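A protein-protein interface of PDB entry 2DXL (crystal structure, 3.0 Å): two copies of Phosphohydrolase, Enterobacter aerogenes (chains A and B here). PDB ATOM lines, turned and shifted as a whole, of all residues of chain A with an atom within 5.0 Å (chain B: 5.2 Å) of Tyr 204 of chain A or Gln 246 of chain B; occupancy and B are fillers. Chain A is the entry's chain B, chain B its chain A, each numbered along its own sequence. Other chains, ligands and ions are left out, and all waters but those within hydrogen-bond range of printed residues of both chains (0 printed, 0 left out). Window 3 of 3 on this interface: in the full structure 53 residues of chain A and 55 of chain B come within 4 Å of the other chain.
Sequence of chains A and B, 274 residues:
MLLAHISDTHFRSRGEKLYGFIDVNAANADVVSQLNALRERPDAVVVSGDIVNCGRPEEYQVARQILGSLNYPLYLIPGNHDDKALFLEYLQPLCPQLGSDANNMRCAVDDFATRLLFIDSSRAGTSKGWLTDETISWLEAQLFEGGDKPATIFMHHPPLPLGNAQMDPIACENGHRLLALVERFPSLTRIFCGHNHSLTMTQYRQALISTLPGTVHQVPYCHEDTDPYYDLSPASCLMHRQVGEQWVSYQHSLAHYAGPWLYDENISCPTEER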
ATOM      1  N   LEU A 160      34.542  12.979  -5.385  1.00  0.00           N
ATOM      2  CA  LEU A 160      34.015  14.153  -4.687  1.00  0.00           C
ATOM      3  C   LEU A 160      34.034  13.964  -3.176  1.00  0.00           C
ATOM      4  O   LEU A 160      34.169  12.825  -2.686  1.00  0.00           O
ATOM      5  CB  LEU A 160      32.601  14.494  -5.167  1.00  0.00           C
ATOM      6  CG  LEU A 160      31.429  13.663  -4.631  1.00  0.00           C
ATOM      7  CD1 LEU A 160      30.088  14.307  -4.988  1.00  0.00           C
ATOM      8  CD2 LEU A 160      31.496  12.217  -5.128  1.00  0.00           C
ATOM      9  N   LEU A 179      33.690  14.370 -12.498  1.00  0.00           N
ATOM     10  CA  LEU A 179      32.339  14.920 -12.401  1.00  0.00           C
ATOM     11  C   LEU A 179      31.882  15.590 -13.716  1.00  0.00           C
ATOM     12  O   LEU A 179      30.738  15.400 -14.163  1.00  0.00           O
ATOM     13  CB  LEU A 179      32.283  15.922 -11.245  1.00  0.00           C
ATOM     14  CG  LEU A 179      31.713  15.567  -9.865  1.00  0.00           C
ATOM     15  CD1 LEU A 179      31.928  14.109  -9.470  1.00  0.00           C
ATOM     16  CD2 LEU A 179      32.306  16.503  -8.815  1.00  0.00           C
ATOM     17  N   VAL A 182      31.050  13.042 -16.230  1.00  0.00           N
ATOM     18  CA  VAL A 182      29.722  12.435 -16.031  1.00  0.00           C
ATOM     19  C   VAL A 182      28.637  13.355 -16.566  1.00  0.00           C
ATOM     20  O   VAL A 182      27.644  12.877 -17.119  1.00  0.00           O
ATOM     21  CB  VAL A 182      29.386  11.956 -14.555  1.00  0.00           C
ATOM     22  CG1 VAL A 182      30.642  11.784 -13.701  1.00  0.00           C
ATOM     23  CG2 VAL A 182      28.370  12.871 -13.867  1.00  0.00           C
ATOM     24  N   GLU A 183      28.829  14.668 -16.417  1.00  0.00           N
ATOM     25  CA  GLU A 183      27.929  15.638 -17.051  1.00  0.00           C
ATOM     26  C   GLU A 183      27.945  15.460 -18.561  1.00  0.00           C
ATOM     27  O   GLU A 183      26.906  15.483 -19.189  1.00  0.00           O
ATOM     28  CB  GLU A 183      28.296  17.071 -16.670  1.00  0.00           C
ATOM     29  CG  GLU A 183      27.798  17.487 -15.299  1.00  0.00           C
ATOM     30  CD  GLU A 183      28.311  18.850 -14.854  1.00  0.00           C
ATOM     31  OE1 GLU A 183      28.538  19.021 -13.640  1.00  0.00           O
ATOM     32  OE2 GLU A 183      28.492  19.750 -15.703  1.00  0.00           O
ATOM     33  N   THR A 202      26.541   7.760  -3.188  1.00  0.00           N
ATOM     34  CA  THR A 202      25.909   8.997  -3.604  1.00  0.00           C
ATOM     35  C   THR A 202      25.569   8.978  -5.108  1.00  0.00           C
ATOM     36  O   THR A 202      25.948   8.047  -5.828  1.00  0.00           O
ATOM     37  CB  THR A 202      26.792  10.203  -3.216  1.00  0.00           C
ATOM     38  OG1 THR A 202      25.990  11.384  -3.134  1.00  0.00           O
ATOM     39  CG2 THR A 202      27.958  10.392  -4.202  1.00  0.00           C
ATOM     40  N   GLN A 203      24.835   9.994  -5.559  1.00  0.00           N
ATOM     41  CA  GLN A 203      24.445  10.123  -6.965  1.00  0.00           C
ATOM     42  C   GLN A 203      24.780  11.503  -7.519  1.00  0.00           C
ATOM     43  O   GLN A 203      24.513  12.531  -6.890  1.00  0.00           O
ATOM     44  CB  GLN A 203      22.945   9.819  -7.160  1.00  0.00           C
ATOM     45  CG  GLN A 203      22.288  10.375  -8.461  1.00  0.00           C
ATOM     46  CD  GLN A 203      21.639  11.793  -8.337  1.00  0.00           C
ATOM     47  OE1 GLN A 203      21.668  12.427  -7.274  1.00  0.00           O
ATOM     48  NE2 GLN A 203      21.049  12.275  -9.443  1.00  0.00           N
ATOM     49  N   TYR A 204      25.362  11.505  -8.711  1.00  0.00           N
ATOM     50  CA  TYR A 204      25.591  12.729  -9.458  1.00  0.00           C
ATOM     51  C   TYR A 204      24.975  12.523 -10.832  1.00  0.00           C
ATOM     52  O   TYR A 204      25.493  11.738 -11.633  1.00  0.00           O
ATOM     53  CB  TYR A 204      27.087  13.024  -9.557  1.00  0.00           C
ATOM     54  CG  TYR A 204      27.382  14.432  -9.985  1.00  0.00           C
ATOM     55  CD1 TYR A 204      27.538  15.449  -9.042  1.00  0.00           C
ATOM     56  CD2 TYR A 204      27.492  14.762 -11.342  1.00  0.00           C
ATOM     57  CE1 TYR A 204      27.804  16.766  -9.443  1.00  0.00           C
ATOM     58  CE2 TYR A 204      27.751  16.072 -11.757  1.00  0.00           C
ATOM     59  CZ  TYR A 204      27.908  17.067 -10.801  1.00  0.00           C
ATOM     60  OH  TYR A 204      28.177  18.359 -11.197  1.00  0.00           O
ATOM     61  N   ARG A 205      23.863  13.211 -11.095  1.00  0.00           N
ATOM     62  CA  ARG A 205      23.092  13.001 -12.323  1.00  0.00           C
ATOM     63  C   ARG A 205      22.809  11.503 -12.549  1.00  0.00           C
ATOM     64  O   ARG A 205      22.152  10.865 -11.718  1.00  0.00           O
ATOM     65  CB  ARG A 205      23.787  13.620 -13.548  1.00  0.00           C
ATOM     66  CG  ARG A 205      24.687  14.826 -13.265  1.00  0.00           C
ATOM     67  CD  ARG A 205      23.913  16.088 -12.966  1.00  0.00           C
ATOM     68  NE  ARG A 205      23.933  16.999 -14.107  1.00  0.00           N
ATOM     69  CZ  ARG A 205      24.492  18.206 -14.096  1.00  0.00           C
ATOM     70  NH1 ARG A 205      25.071  18.661 -12.992  1.00  0.00           N
ATOM     71  NH2 ARG A 205      24.458  18.963 -15.185  1.00  0.00           N
ATOM     72  N   GLN A 206      23.311  10.938 -13.650  1.00  0.00           N
ATOM     73  CA  GLN A 206      23.052   9.524 -13.979  1.00  0.00           C
ATOM     74  C   GLN A 206      23.977   8.586 -13.234  1.00  0.00           C
ATOM     75  O   GLN A 206      23.858   7.382 -13.379  1.00  0.00           O
ATOM     76  CB  GLN A 206      23.234   9.231 -15.473  1.00  0.00           C
ATOM     77  CG  GLN A 206      23.448  10.438 -16.371  1.00  0.00           C
ATOM     78  CD  GLN A 206      24.879  10.958 -16.355  1.00  0.00           C
ATOM     79  OE1 GLN A 206      25.838  10.208 -16.170  1.00  0.00           O
ATOM     80  NE2 GLN A 206      25.025  12.259 -16.570  1.00  0.00           N
ATOM     81  N   ALA A 207      24.917   9.121 -12.467  1.00  0.00           N
ATOM     82  CA  ALA A 207      25.967   8.283 -11.923  1.00  0.00           C
ATOM     83  C   ALA A 207      25.807   7.985 -10.436  1.00  0.00           C
ATOM     84  O   ALA A 207      25.760   8.895  -9.603  1.00  0.00           O
ATOM     85  CB  ALA A 207      27.323   8.875 -12.208  1.00  0.00           C
ATOM     86  N   ILE A 209      27.700   6.731  -7.407  1.00  0.00           N
ATOM     87  CA  ILE A 209      29.095   6.740  -6.973  1.00  0.00           C
ATOM     88  C   ILE A 209      29.215   6.207  -5.541  1.00  0.00           C
ATOM     89  O   ILE A 209      28.592   6.747  -4.622  1.00  0.00           O
ATOM     90  CB  ILE A 209      29.677   8.153  -6.994  1.00  0.00           C
ATOM     91  CG1 ILE A 209      29.491   8.798  -8.368  1.00  0.00           C
ATOM     92  CG2 ILE A 209      31.146   8.115  -6.605  1.00  0.00           C
ATOM     93  CD1 ILE A 209      29.748  10.294  -8.381  1.00  0.00           C
ATOM     94  N   GLN B 203      20.833   2.131  -9.903  1.00  0.00           N
ATOM     95  CA  GLN B 203      20.294   3.428 -10.301  1.00  0.00           C
ATOM     96  C   GLN B 203      19.388   3.303 -11.492  1.00  0.00           C
ATOM     97  O   GLN B 203      19.620   2.494 -12.385  1.00  0.00           O
ATOM     98  CB  GLN B 203      21.375   4.469 -10.601  1.00  0.00           C
ATOM     99  CG  GLN B 203      21.583   5.472  -9.462  1.00  0.00           C
ATOM    100  CD  GLN B 203      21.994   6.889  -9.921  1.00  0.00           C
ATOM    101  OE1 GLN B 203      21.602   7.358 -10.999  1.00  0.00           O
ATOM    102  NE2 GLN B 203      22.774   7.576  -9.081  1.00  0.00           N
ATOM    103  N   ARG B 241      23.165  11.803   5.233  1.00  0.00           N
ATOM    104  CA  ARG B 241      23.569  13.166   5.550  1.00  0.00           C
ATOM    105  C   ARG B 241      23.555  14.057   4.325  1.00  0.00           C
ATOM    106  O   ARG B 241      23.948  13.626   3.235  1.00  0.00           O
ATOM    107  CB  ARG B 241      24.956  13.213   6.199  1.00  0.00           C
ATOM    108  CG  ARG B 241      25.291  14.583   6.778  1.00  0.00           C
ATOM    109  CD  ARG B 241      26.738  14.731   7.157  1.00  0.00           C
ATOM    110  NE  ARG B 241      27.058  13.893   8.313  1.00  0.00           N
ATOM    111  CZ  ARG B 241      27.008  14.300   9.585  1.00  0.00           C
ATOM    112  NH1 ARG B 241      26.650  15.563   9.873  1.00  0.00           N
ATOM    113  NH2 ARG B 241      27.327  13.437  10.564  1.00  0.00           N
ATOM    114  N   GLN B 242      23.103  15.297   4.518  1.00  0.00           N
ATOM    115  CA  GLN B 242      23.166  16.317   3.486  1.00  0.00           C
ATOM    116  C   GLN B 242      24.533  16.987   3.536  1.00  0.00           C
ATOM    117  O   GLN B 242      24.896  17.558   4.562  1.00  0.00           O
ATOM    118  CB  GLN B 242      22.084  17.357   3.727  1.00  0.00           C
ATOM    119  CG  GLN B 242      21.928  18.363   2.607  1.00  0.00           C
ATOM    120  CD  GLN B 242      21.153  17.805   1.423  1.00  0.00           C
ATOM    121  OE1 GLN B 242      21.608  17.903   0.274  1.00  0.00           O
ATOM    122  NE2 GLN B 242      19.971  17.220   1.695  1.00  0.00           N
ATOM    123  N   VAL B 243      25.294  16.899   2.440  1.00  0.00           N
ATOM    124  CA  VAL B 243      26.630  17.517   2.342  1.00  0.00           C
ATOM    125  C   VAL B 243      26.689  18.463   1.130  1.00  0.00           C
ATOM    126  O   VAL B 243      26.931  18.021   0.002  1.00  0.00           O
ATOM    127  CB  VAL B 243      27.767  16.458   2.240  1.00  0.00           C
ATOM    128  CG1 VAL B 243      29.137  17.120   2.412  1.00  0.00           C
ATOM    129  CG2 VAL B 243      27.585  15.344   3.267  1.00  0.00           C
ATOM    130  N   GLY B 244      26.469  19.756   1.362  1.00  0.00           N
ATOM    131  CA  GLY B 244      26.252  20.674   0.260  1.00  0.00           C
ATOM    132  C   GLY B 244      25.118  20.164  -0.610  1.00  0.00           C
ATOM    133  O   GLY B 244      24.049  19.815  -0.104  1.00  0.00           O
ATOM    134  N   GLU B 245      25.363  20.087  -1.914  1.00  0.00           N
ATOM    135  CA  GLU B 245      24.351  19.622  -2.868  1.00  0.00           C
ATOM    136  C   GLU B 245      24.141  18.115  -2.894  1.00  0.00           C
ATOM    137  O   GLU B 245      23.261  17.624  -3.601  1.00  0.00           O
ATOM    138  CB  GLU B 245      24.693  20.088  -4.280  1.00  0.00           C
ATOM    139  CG  GLU B 245      23.640  20.978  -4.908  1.00  0.00           C
ATOM    140  CD  GLU B 245      23.513  22.323  -4.220  1.00  0.00           C
ATOM    141  OE1 GLU B 245      22.462  22.981  -4.413  1.00  0.00           O
ATOM    142  OE2 GLU B 245      24.456  22.721  -3.491  1.00  0.00           O
ATOM    143  N   GLN B 246      24.951  17.387  -2.134  1.00  0.00           N
ATOM    144  CA  GLN B 246      24.926  15.935  -2.171  1.00  0.00           C
ATOM    145  C   GLN B 246      24.163  15.335  -1.008  1.00  0.00           C
ATOM    146  O   GLN B 246      24.307  15.772   0.131  1.00  0.00           O
ATOM    147  CB  GLN B 246      26.351  15.380  -2.183  1.00  0.00           C
ATOM    148  CG  GLN B 246      27.188  15.827  -3.367  1.00  0.00           C
ATOM    149  CD  GLN B 246      26.560  15.466  -4.705  1.00  0.00           C
ATOM    150  OE1 GLN B 246      26.089  14.344  -4.902  1.00  0.00           O
ATOM    151  NE2 GLN B 246      26.558  16.422  -5.635  1.00  0.00           N
ATOM    152  N   TRP B 247      23.339  14.338  -1.317  1.00  0.00           N
ATOM    153  CA  TRP B 247      22.837  13.396  -0.331  1.00  0.00           C
ATOM    154  C   TRP B 247      23.822  12.231  -0.296  1.00  0.00           C
ATOM    155  O   TRP B 247      24.028  11.554  -1.306  1.00  0.00           O
ATOM    156  CB  TRP B 247      21.453  12.908  -0.743  1.00  0.00           C
ATOM    157  CG  TRP B 247      20.827  11.884   0.163  1.00  0.00           C
ATOM    158  CD1 TRP B 247      21.249  10.591   0.388  1.00  0.00           C
ATOM    159  CD2 TRP B 247      19.641  12.053   0.941  1.00  0.00           C
ATOM    160  NE1 TRP B 247      20.402   9.960   1.271  1.00  0.00           N
ATOM    161  CE2 TRP B 247      19.406  10.834   1.623  1.00  0.00           C
ATOM    162  CE3 TRP B 247      18.756  13.119   1.139  1.00  0.00           C
ATOM    163  CZ2 TRP B 247      18.313  10.656   2.472  1.00  0.00           C
ATOM    164  CZ3 TRP B 247      17.668  12.937   1.987  1.00  0.00           C
ATOM    165  CH2 TRP B 247      17.459  11.718   2.643  1.00  0.00           C
ATOM    166  N   VAL B 248      24.447  12.004   0.850  1.00  0.00           N
ATOM    167  CA  VAL B 248      25.322  10.838   0.996  1.00  0.00           C
ATOM    168  C   VAL B 248      24.793   9.892   2.052  1.00  0.00           C
ATOM    169  O   VAL B 248      24.310  10.314   3.111  1.00  0.00           O
ATOM    170  CB  VAL B 248      26.786  11.203   1.339  1.00  0.00           C
ATOM    171  CG1 VAL B 248      27.430  11.993   0.195  1.00  0.00           C
ATOM    172  CG2 VAL B 248      26.827  12.021   2.605  1.00  0.00           C
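Along chain A the printed residues that touch a printed residue of chain B span positions 160 to 207. Among the printed residues, no Asp or Glu carboxylate lies within 4 Å of a Lys or Arg side-chain nitrogen of the other chain.
The backbone NH (N) of Arg 241 of chain B lies within hydrogen-bond range of the backbone carbonyl oxygen (O) of Val 248 of chain B, 2.8 Å away. OE1 of Gln 242 of chain B lies close to O of Gln 246 of chain B (3.4 Å). The side-chain carboxylate (OE1) of Glu 183 of chain A is in hydrogen-bond range of the side-chain hydroxyl (OH) of Tyr 204 of chain A, 2.6 Å away. The side-chain carboxylate of Glu 183 of chain A is in salt-bridge range of the guanidinium group of Arg 205 of chain A (3.5 Å). The backbone NH of Thr 202 of chain A sits at hydrogen-bond distance from the backbone carbonyl oxygen of Ile 209 of chain A, 2.7 Å away. NE2 of Gln 203 of chain A is in hydrogen-bond range of O of Arg 205 of chain A, at 2.9 Å.
The side-chain amide oxygen (OE1) of Gln 203 of chain B sits close to the backbone carbonyl oxygen (O) of Gln 206 of chain A (3.3 Å). The backbone carbonyl oxygen (O) of Ala 207 of chain A lies within hydrogen-bond range of the side-chain amide nitrogen (NE2) of Gln 203 of chain B, at 3.3 Å. The side-chain amide oxygen of Gln 246 of chain B is in hydrogen-bond range of the side-chain hydroxyl of Thr 202 of chain A (3.4 Å). The side-chain amide oxygen (OE1) of Gln 246 of chain B lies close to the backbone carbonyl oxygen (O) of Gln 203 of chain A (3.1 Å). The backbone carbonyl oxygen (O) of Trp 247 of chain B is in hydrogen-bond range of the side-chain hydroxyl (OG1) of Thr 202 of chain A (2.7 Å).
Gln 203 of chain A touches its own counterpart, Gln 203 of chain B.
Of chain B, only Gln 246 comes within 4 Å of Tyr 204 of chain A. Gln 246 of chain B touches just these residues of chain A: Leu 160 (3.7 Å), Thr 202 (3.4 Å), Gln 203 (3.1 Å) and Tyr 204 (3.7 Å). Printed residues of chain B within 4 Å of Leu 160 of chain A: Gln 246 (3.7 Å). Printed residues of chain B within 4 Å of Ala 207 of chain A: Gln 203. Of the printed residues of chain B, Thr 202 of chain A touches Gln 246 (3.4 Å), Trp 247 (2.7 Å) and Val 248 (3.7 Å). Of the printed residues of chain B, Gln 203 of chain A touches Gln 203 (2.9 Å) and Gln 246 (3.1 Å). Of the printed residues of chain A, Gln 203 of chain B touches Gln 203 (2.9 Å), Arg 205 (3.6 Å), Gln 206 (3.3 Å) and Ala 207 (3.3 Å). Leu 179 of chain A touches none of the printed residues of chain B.
CG of Gln 246 of chain B touches CD1 of Leu 160 of chain A (3.7 Å). Val 248 of chain B touches Thr 202 of chain A. Gln 203 of chain A touches Gln 203 of chain B (CG to NE2, 2.9 Å). NE2 of Gln 246 of chain B touches CD1 of Tyr 204 of chain A (3.7 Å). O of Arg 205 of chain A touches OE1 of Gln 203 of chain B, at 3.6 Å.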
